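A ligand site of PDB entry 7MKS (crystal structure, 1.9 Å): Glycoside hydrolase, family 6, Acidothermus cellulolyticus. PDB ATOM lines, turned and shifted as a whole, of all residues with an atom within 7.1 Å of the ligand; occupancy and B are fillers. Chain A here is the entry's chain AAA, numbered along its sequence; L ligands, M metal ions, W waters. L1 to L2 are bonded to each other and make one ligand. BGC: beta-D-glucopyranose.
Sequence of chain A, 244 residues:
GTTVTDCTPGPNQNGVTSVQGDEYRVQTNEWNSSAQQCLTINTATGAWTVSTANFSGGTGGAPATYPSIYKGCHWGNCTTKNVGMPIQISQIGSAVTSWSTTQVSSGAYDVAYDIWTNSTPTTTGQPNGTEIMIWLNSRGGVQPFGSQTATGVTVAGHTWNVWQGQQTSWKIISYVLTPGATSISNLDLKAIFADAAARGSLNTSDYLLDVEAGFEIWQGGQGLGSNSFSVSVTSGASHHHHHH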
ATOM      1  N   TRP A  31     -25.243 -12.265   9.237  1.00  0.00           N
ATOM      2  CA  TRP A  31     -26.279 -12.440   8.214  1.00  0.00           C
ATOM      3  C   TRP A  31     -27.681 -12.249   8.778  1.00  0.00           C
ATOM      4  O   TRP A  31     -28.604 -12.162   7.986  1.00  0.00           O
ATOM      5  CB  TRP A  31     -26.105 -13.802   7.546  1.00  0.00           C
ATOM      6  CG  TRP A  31     -26.315 -14.974   8.415  1.00  0.00           C
ATOM      7  CD1 TRP A  31     -25.349 -15.648   9.102  1.00  0.00           C
ATOM      8  CD2 TRP A  31     -27.555 -15.684   8.626  1.00  0.00           C
ATOM      9  NE1 TRP A  31     -25.917 -16.740   9.707  1.00  0.00           N
ATOM     10  CE2 TRP A  31     -27.252 -16.768   9.455  1.00  0.00           C
ATOM     11  CE3 TRP A  31     -28.868 -15.519   8.178  1.00  0.00           C
ATOM     12  CZ2 TRP A  31     -28.219 -17.703   9.877  1.00  0.00           C
ATOM     13  CZ3 TRP A  31     -29.837 -16.424   8.607  1.00  0.00           C
ATOM     14  CH2 TRP A  31     -29.509 -17.502   9.420  1.00  0.00           C
ATOM     15  N   GLY A  58     -33.288 -14.929  21.883  1.00  0.00           N
ATOM     16  CA  GLY A  58     -33.562 -16.274  22.366  1.00  0.00           C
ATOM     17  C   GLY A  58     -32.506 -17.230  21.836  1.00  0.00           C
ATOM     18  O   GLY A  58     -31.719 -16.831  20.964  1.00  0.00           O
ATOM     19  N   THR A  59     -32.532 -18.464  22.292  1.00  0.00           N
ATOM     20  CA  THR A  59     -31.526 -19.481  21.907  1.00  0.00           C
ATOM     21  C   THR A  59     -32.103 -20.421  20.849  1.00  0.00           C
ATOM     22  O   THR A  59     -31.363 -21.342  20.408  1.00  0.00           O
ATOM     23  CB  THR A  59     -31.054 -20.199  23.144  1.00  0.00           C
ATOM     24  OG1 THR A  59     -32.234 -20.703  23.765  1.00  0.00           O
ATOM     25  CG2 THR A  59     -30.274 -19.275  24.059  1.00  0.00           C
ATOM     26  N   GLY A  60     -33.368 -20.245  20.498  1.00  0.00           N
ATOM     27  CA  GLY A  60     -34.029 -21.074  19.464  1.00  0.00           C
ATOM     28  C   GLY A  60     -33.906 -20.428  18.106  1.00  0.00           C
ATOM     29  O   GLY A  60     -33.606 -19.212  18.048  1.00  0.00           O
ATOM     30  N   GLY A  61     -34.087 -21.189  17.032  1.00  0.00           N
ATOM     31  CA  GLY A  61     -34.156 -20.590  15.697  1.00  0.00           C
ATOM     32  C   GLY A  61     -32.791 -20.135  15.212  1.00  0.00           C
ATOM     33  O   GLY A  61     -31.764 -20.651  15.695  1.00  0.00           O
ATOM     34  N   ALA A  62     -32.783 -19.196  14.288  1.00  0.00           N
ATOM     35  CA  ALA A  62     -31.539 -18.768  13.625  1.00  0.00           C
ATOM     36  C   ALA A  62     -30.683 -17.980  14.608  1.00  0.00           C
ATOM     37  O   ALA A  62     -31.182 -17.217  15.441  1.00  0.00           O
ATOM     38  CB  ALA A  62     -31.807 -17.974  12.372  1.00  0.00           C
ATOM     39  N   PRO A  63     -29.344 -18.110  14.473  1.00  0.00           N
ATOM     40  CA  PRO A  63     -28.432 -17.254  15.211  1.00  0.00           C
ATOM     41  C   PRO A  63     -28.487 -15.837  14.622  1.00  0.00           C
ATOM     42  O   PRO A  63     -29.086 -15.635  13.546  1.00  0.00           O
ATOM     43  CB  PRO A  63     -27.084 -17.959  14.978  1.00  0.00           C
ATOM     44  CG  PRO A  63     -27.223 -18.524  13.552  1.00  0.00           C
ATOM     45  CD  PRO A  63     -28.658 -19.023  13.539  1.00  0.00           C
ATOM     46  N   ASP A 110     -22.403 -21.631  19.215  1.00  0.00           N
ATOM     47  CA  ASP A 110     -21.676 -22.865  18.829  1.00  0.00           C
ATOM     48  C   ASP A 110     -20.302 -22.488  18.273  1.00  0.00           C
ATOM     49  O   ASP A 110     -20.054 -21.314  17.989  1.00  0.00           O
ATOM     50  CB  ASP A 110     -22.483 -23.776  17.915  1.00  0.00           C
ATOM     51  CG  ASP A 110     -22.803 -23.244  16.525  1.00  0.00           C
ATOM     52  OD1 ASP A 110     -21.961 -22.548  15.938  1.00  0.00           O
ATOM     53  OD2 ASP A 110     -23.957 -23.490  16.063  1.00  0.00           O
ATOM     54  N   ALA A 112     -18.101 -24.017  15.393  1.00  0.00           N
ATOM     55  CA  ALA A 112     -18.473 -24.992  14.378  1.00  0.00           C
ATOM     56  C   ALA A 112     -17.776 -24.721  13.041  1.00  0.00           C
ATOM     57  O   ALA A 112     -17.794 -23.603  12.533  1.00  0.00           O
ATOM     58  CB  ALA A 112     -19.969 -25.001  14.166  1.00  0.00           C
ATOM     59  N   ASP A 114     -18.577 -25.201   9.090  1.00  0.00           N
ATOM     60  CA  ASP A 114     -19.693 -25.144   8.120  1.00  0.00           C
ATOM     61  C   ASP A 114     -19.097 -25.454   6.739  1.00  0.00           C
ATOM     62  O   ASP A 114     -18.185 -24.716   6.293  1.00  0.00           O
ATOM     63  CB  ASP A 114     -20.339 -23.776   8.155  1.00  0.00           C
ATOM     64  CG  ASP A 114     -21.831 -23.778   7.802  1.00  0.00           C
ATOM     65  OD1 ASP A 114     -22.482 -24.842   7.991  1.00  0.00           O
ATOM     66  OD2 ASP A 114     -22.344 -22.683   7.403  1.00  0.00           O
ATOM     67  N   GLU A 131     -25.060 -29.187   3.721  1.00  0.00           N
ATOM     68  CA  GLU A 131     -24.314 -28.397   4.722  1.00  0.00           C
ATOM     69  C   GLU A 131     -23.858 -29.383   5.803  1.00  0.00           C
ATOM     70  O   GLU A 131     -24.713 -30.000   6.436  1.00  0.00           O
ATOM     71  CB  GLU A 131     -25.221 -27.331   5.314  1.00  0.00           C
ATOM     72  CG  GLU A 131     -24.471 -26.374   6.175  1.00  0.00           C
ATOM     73  CD  GLU A 131     -25.373 -25.399   6.892  1.00  0.00           C
ATOM     74  OE1 GLU A 131     -26.629 -25.432   6.630  1.00  0.00           O
ATOM     75  OE2 GLU A 131     -24.852 -24.623   7.692  1.00  0.00           O
ATOM     76  N   MET A 133     -22.011 -29.546   9.301  1.00  0.00           N
ATOM     77  CA  MET A 133     -21.531 -28.742  10.422  1.00  0.00           C
ATOM     78  C   MET A 133     -20.736 -29.696  11.325  1.00  0.00           C
ATOM     79  O   MET A 133     -21.113 -30.879  11.465  1.00  0.00           O
ATOM     80  CB  MET A 133     -22.622 -28.030  11.223  1.00  0.00           C
ATOM     81  CG  MET A 133     -23.373 -27.015  10.408  1.00  0.00           C
ATOM     82  SD  MET A 133     -24.194 -25.820  11.442  1.00  0.00           S
ATOM     83  CE  MET A 133     -22.924 -24.562  11.565  1.00  0.00           C
ATOM     84  N   TRP A 135     -19.486 -29.422  15.202  1.00  0.00           N
ATOM     85  CA  TRP A 135     -19.588 -28.605  16.423  1.00  0.00           C
ATOM     86  C   TRP A 135     -18.485 -29.063  17.379  1.00  0.00           C
ATOM     87  O   TRP A 135     -18.676 -30.116  17.980  1.00  0.00           O
ATOM     88  CB  TRP A 135     -20.958 -28.689  17.089  1.00  0.00           C
ATOM     89  CG  TRP A 135     -22.121 -28.022  16.396  1.00  0.00           C
ATOM     90  CD1 TRP A 135     -22.299 -27.788  15.062  1.00  0.00           C
ATOM     91  CD2 TRP A 135     -23.281 -27.483  17.045  1.00  0.00           C
ATOM     92  NE1 TRP A 135     -23.477 -27.117  14.854  1.00  0.00           N
ATOM     93  CE2 TRP A 135     -24.102 -26.925  16.055  1.00  0.00           C
ATOM     94  CE3 TRP A 135     -23.698 -27.444  18.383  1.00  0.00           C
ATOM     95  CZ2 TRP A 135     -25.320 -26.290  16.369  1.00  0.00           C
ATOM     96  CZ3 TRP A 135     -24.877 -26.834  18.692  1.00  0.00           C
ATOM     97  CH2 TRP A 135     -25.651 -26.223  17.699  1.00  0.00           C
ATOM     98  N   GLY A 141     -27.576 -23.440  25.775  1.00  0.00           N
ATOM     99  CA  GLY A 141     -28.884 -24.077  25.460  1.00  0.00           C
ATOM    100  C   GLY A 141     -29.170 -24.209  23.981  1.00  0.00           C
ATOM    101  O   GLY A 141     -30.298 -24.537  23.603  1.00  0.00           O
ATOM    102  N   VAL A 142     -28.239 -23.851  23.110  1.00  0.00           N
ATOM    103  CA  VAL A 142     -28.497 -23.976  21.657  1.00  0.00           C
ATOM    104  C   VAL A 142     -28.390 -25.451  21.257  1.00  0.00           C
ATOM    105  O   VAL A 142     -27.770 -26.248  21.928  1.00  0.00           O
ATOM    106  CB  VAL A 142     -27.545 -23.081  20.823  1.00  0.00           C
ATOM    107  CG1 VAL A 142     -27.780 -21.630  21.167  1.00  0.00           C
ATOM    108  CG2 VAL A 142     -26.096 -23.475  20.989  1.00  0.00           C
ATOM    109  N   GLN A 143     -29.004 -25.830  20.139  1.00  0.00           N
ATOM    110  CA  GLN A 143     -28.872 -27.185  19.596  1.00  0.00           C
ATOM    111  C   GLN A 143     -28.861 -27.061  18.085  1.00  0.00           C
ATOM    112  O   GLN A 143     -29.263 -26.045  17.491  1.00  0.00           O
ATOM    113  CB  GLN A 143     -29.993 -28.102  20.124  1.00  0.00           C
ATOM    114  CG  GLN A 143     -31.344 -27.772  19.525  1.00  0.00           C
ATOM    115  CD  GLN A 143     -32.484 -28.625  20.066  1.00  0.00           C
ATOM    116  OE1 GLN A 143     -33.363 -29.134  19.334  1.00  0.00           O
ATOM    117  NE2 GLN A 143     -32.495 -28.724  21.379  1.00  0.00           N
ATOM    118  N   PRO A 144     -28.396 -28.131  17.428  1.00  0.00           N
ATOM    119  CA  PRO A 144     -28.346 -28.177  15.992  1.00  0.00           C
ATOM    120  C   PRO A 144     -29.719 -28.168  15.338  1.00  0.00           C
ATOM    121  O   PRO A 144     -30.734 -28.420  15.986  1.00  0.00           O
ATOM    122  CB  PRO A 144     -27.589 -29.479  15.683  1.00  0.00           C
ATOM    123  CG  PRO A 144     -26.918 -29.824  16.968  1.00  0.00           C
ATOM    124  CD  PRO A 144     -27.838 -29.346  18.042  1.00  0.00           C
ATOM    125  N   PHE A 145     -29.702 -27.906  14.037  1.00  0.00           N
ATOM    126  CA  PHE A 145     -30.896 -28.009  13.170  1.00  0.00           C
ATOM    127  C   PHE A 145     -31.311 -29.465  13.040  1.00  0.00           C
ATOM    128  O   PHE A 145     -30.459 -30.367  12.963  1.00  0.00           O
ATOM    129  CB  PHE A 145     -30.566 -27.442  11.784  1.00  0.00           C
ATOM    130  CG  PHE A 145     -31.759 -27.123  10.939  1.00  0.00           C
ATOM    131  CD1 PHE A 145     -32.305 -28.059  10.101  1.00  0.00           C
ATOM    132  CD2 PHE A 145     -32.305 -25.863  10.941  1.00  0.00           C
ATOM    133  CE1 PHE A 145     -33.414 -27.764   9.302  1.00  0.00           C
ATOM    134  CE2 PHE A 145     -33.376 -25.537  10.118  1.00  0.00           C
ATOM    135  CZ  PHE A 145     -33.952 -26.491   9.321  1.00  0.00           C
ATOM    136  N   GLY A 146     -32.625 -29.689  12.975  1.00  0.00           N
ATOM    137  CA  GLY A 146     -33.228 -30.989  12.723  1.00  0.00           C
ATOM    138  C   GLY A 146     -33.350 -31.810  13.983  1.00  0.00           C
ATOM    139  O   GLY A 146     -33.758 -31.280  15.039  1.00  0.00           O
ATOM    140  N   GLN A 167     -33.236 -28.488   4.976  1.00  0.00           N
ATOM    141  CA  GLN A 167     -33.460 -27.062   4.727  1.00  0.00           C
ATOM    142  C   GLN A 167     -34.225 -26.881   3.427  1.00  0.00           C
ATOM    143  O   GLN A 167     -34.552 -27.855   2.762  1.00  0.00           O
ATOM    144  CB  GLN A 167     -32.103 -26.345   4.755  1.00  0.00           C
ATOM    145  CG  GLN A 167     -31.851 -25.686   6.108  1.00  0.00           C
ATOM    146  CD  GLN A 167     -32.675 -24.436   6.295  1.00  0.00           C
ATOM    147  OE1 GLN A 167     -33.644 -24.080   5.566  1.00  0.00           O
ATOM    148  NE2 GLN A 167     -32.200 -23.684   7.259  1.00  0.00           N
ATOM    149  N   ILE A 172     -28.923 -30.830   5.771  1.00  0.00           N
ATOM    150  CA  ILE A 172     -27.934 -30.510   6.810  1.00  0.00           C
ATOM    151  C   ILE A 172     -27.637 -31.738   7.653  1.00  0.00           C
ATOM    152  O   ILE A 172     -28.536 -32.501   8.016  1.00  0.00           O
ATOM    153  CB  ILE A 172     -28.310 -29.246   7.619  1.00  0.00           C
ATOM    154  CG1 ILE A 172     -27.203 -28.889   8.628  1.00  0.00           C
ATOM    155  CG2 ILE A 172     -29.635 -29.365   8.341  1.00  0.00           C
ATOM    156  CD1 ILE A 172     -27.433 -27.526   9.284  1.00  0.00           C
ATOM    157  N   SER A 174     -25.159 -32.296  11.198  1.00  0.00           N
ATOM    158  CA  SER A 174     -24.296 -31.680  12.224  1.00  0.00           C
ATOM    159  C   SER A 174     -23.686 -32.793  13.103  1.00  0.00           C
ATOM    160  O   SER A 174     -24.464 -33.568  13.761  1.00  0.00           O
ATOM    161  CB  SER A 174     -25.024 -30.634  13.047  1.00  0.00           C
ATOM    162  OG  SER A 174     -25.630 -29.614  12.234  1.00  0.00           O
ATOM    163  N   GLU A 216     -21.522 -19.540  15.444  1.00  0.00           N
ATOM    164  CA  GLU A 216     -22.923 -19.043  15.333  1.00  0.00           C
ATOM    165  C   GLU A 216     -23.262 -18.497  16.728  1.00  0.00           C
ATOM    166  O   GLU A 216     -23.103 -19.214  17.689  1.00  0.00           O
ATOM    167  CB  GLU A 216     -23.915 -20.120  14.917  1.00  0.00           C
ATOM    168  CG  GLU A 216     -23.583 -20.767  13.606  1.00  0.00           C
ATOM    169  CD  GLU A 216     -24.698 -21.718  13.196  1.00  0.00           C
ATOM    170  OE1 GLU A 216     -24.794 -22.817  13.778  1.00  0.00           O
ATOM    171  OE2 GLU A 216     -25.541 -21.319  12.338  1.00  0.00           O
ATOM    172  N   TRP A 218     -25.978 -16.540  19.304  1.00  0.00           N
ATOM    173  CA  TRP A 218     -27.358 -16.145  19.696  1.00  0.00           C
ATOM    174  C   TRP A 218     -27.294 -15.056  20.799  1.00  0.00           C
ATOM    175  O   TRP A 218     -28.137 -14.140  20.763  1.00  0.00           O
ATOM    176  CB  TRP A 218     -28.117 -17.388  20.158  1.00  0.00           C
ATOM    177  CG  TRP A 218     -28.603 -18.316  19.079  1.00  0.00           C
ATOM    178  CD1 TRP A 218     -29.872 -18.400  18.553  1.00  0.00           C
ATOM    179  CD2 TRP A 218     -27.844 -19.349  18.438  1.00  0.00           C
ATOM    180  NE1 TRP A 218     -29.930 -19.416  17.633  1.00  0.00           N
ATOM    181  CE2 TRP A 218     -28.710 -20.011  17.542  1.00  0.00           C
ATOM    182  CE3 TRP A 218     -26.512 -19.768  18.526  1.00  0.00           C
ATOM    183  CZ2 TRP A 218     -28.289 -21.115  16.785  1.00  0.00           C
ATOM    184  CZ3 TRP A 218     -26.107 -20.857  17.789  1.00  0.00           C
ATOM    185  CH2 TRP A 218     -26.983 -21.517  16.932  1.00  0.00           C
HETATM  186  C2  BGC L   1     -34.609 -25.051  16.158  1.00  0.00           C
HETATM  187  C3  BGC L   1     -33.344 -25.298  15.324  1.00  0.00           C
HETATM  188  C4  BGC L   1     -32.215 -24.361  15.714  1.00  0.00           C
HETATM  189  C5  BGC L   1     -31.982 -24.369  17.232  1.00  0.00           C
HETATM  190  C6  BGC L   1     -30.934 -23.354  17.749  1.00  0.00           C
HETATM  191  C1  BGC L   1     -34.262 -25.047  17.649  1.00  0.00           C
HETATM  192  O1  BGC L   1     -35.431 -24.600  18.346  1.00  0.00           O
HETATM  193  O2  BGC L   1     -35.520 -26.131  15.903  1.00  0.00           O
HETATM  194  O3  BGC L   1     -33.609 -25.266  13.918  1.00  0.00           O
HETATM  195  O4  BGC L   1     -31.004 -24.829  15.112  1.00  0.00           O
HETATM  196  O5  BGC L   1     -33.250 -24.011  17.838  1.00  0.00           O
HETATM  197  O6  BGC L   1     -30.728 -23.531  19.182  1.00  0.00           O
HETATM  198  C2  BGC L   2     -28.866 -24.406  14.178  1.00  0.00           C
HETATM  199  C3  BGC L   2     -28.000 -23.550  13.330  1.00  0.00           C
HETATM  200  C4  BGC L   2     -28.743 -23.093  12.086  1.00  0.00           C
HETATM  201  C5  BGC L   2     -30.159 -22.549  12.400  1.00  0.00           C
HETATM  202  C6  BGC L   2     -30.915 -22.101  11.133  1.00  0.00           C
HETATM  203  C1  BGC L   2     -30.284 -23.837  14.424  1.00  0.00           C
HETATM  204  O2  BGC L   2     -28.255 -24.514  15.418  1.00  0.00           O
HETATM  205  O3  BGC L   2     -26.786 -24.243  12.913  1.00  0.00           O
HETATM  206  O4  BGC L   2     -28.015 -22.054  11.521  1.00  0.00           O
HETATM  207  O5  BGC L   2     -30.872 -23.592  13.137  1.00  0.00           O
HETATM  208  O6  BGC L   2     -32.122 -21.430  11.589  1.00  0.00           O
HETATM  209 ZN    ZN M   1     -27.098 -23.604   7.982  1.00  0.00          ZN
HETATM  210  O   HOH W   1     -26.412 -23.762   9.956  1.00  0.00           O
HETATM  211  O   HOH W   2     -34.777 -27.672  13.148  1.00  0.00           O
HETATM  212  O   HOH W   3     -27.087 -27.210  12.980  1.00  0.00           O
HETATM  213  O   HOH W   4     -33.158 -20.348   9.519  1.00  0.00           O
HETATM  214  O   HOH W   5     -37.629 -24.891  14.387  1.00  0.00           O
HETATM  215  O   HOH W   6     -37.157 -27.597  18.546  1.00  0.00           O
HETATM  216  O   HOH W   7     -34.004 -22.780  12.961  1.00  0.00           O
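CA of Gly 60 touches O5 of BGC L1, at 3.4 Å.
Ala 62 touches the ligand.
CD of Pro 63 touches O4 of BGC L2, at 3.7 Å.
CZ2 of Trp 135 touches O2 of BGC L2, 3.6 Å away.
CA of Val 142 touches O6 of BGC L1 (3.4 Å).
Pro 144 touches the ligand.
CD2 of Phe 145 touches O3 of BGC L1, 3.3 Å away.
CH2 of Trp 218 touches O2 of BGC L2 (3.6 Å).
Hydrophobic or aromatic side chains that line the ligand: Ala 62, Pro 63, Met 133, Trp 135, Val 142, Phe 145 and Trp 218.
Within 4 Å of the ligand: Thr 59, Gly 60, Gly 61, Ala 62, Pro 63, Met 133, Trp 135, Val 142, Gln 143, Pro 144, Phe 145, Glu 216 and Trp 218.
O of Thr 59 is in hydrogen-bond range of O6 of BGC L1 (2.6 Å).
The side-chain carboxylate (OE1) of Glu 216 lies within hydrogen-bond range of an oxygen (O3) of BGC L2, at 2.6 Å.
The backbone NH of Gln 143 lies within hydrogen-bond range of an oxygen (O6) of BGC L1 (3.0 Å).
An oxygen (O2) of BGC L2 lies within hydrogen-bond range of the backbone carbonyl oxygen of Gln 143.
An oxygen (O5) of BGC L1 sits at hydrogen-bond distance from the backbone NH of Gly 61, at 3.1 Å.
An oxygen (O3) of BGC L2 sits at hydrogen-bond distance from the side-chain sulfur of Met 133.
Water W2 bridges O3 of BGC L1 (2.8 Å) and N of Gly 146 (3.0 Å).
Water W1 lies within hydrogen-bond range of an oxygen (O4) of BGC L2 (2.8 Å) and the side-chain sulfur (SD) of Met 133 (3.4 Å).
Water W3 lies within hydrogen-bond range of N of Phe 145, OG of Ser 174, O3 of BGC L2 and SD of Met 133.
O of Glu 216 is in hydrogen-bond range of N of Asp 110, at 2.9 Å.
NE1 of Trp 218 lies within hydrogen-bond range of O of Gly 61, 2.9 Å away.
The side-chain sulfur (SD) of Met 133 lies within hydrogen-bond range of the indole nitrogen (NE1) of Trp 135 (3.7 Å).
The backbone carbonyl oxygen (O) of Ala 62 lies within hydrogen-bond range of the indole nitrogen (NE1) of Trp 218 (3.3 Å).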
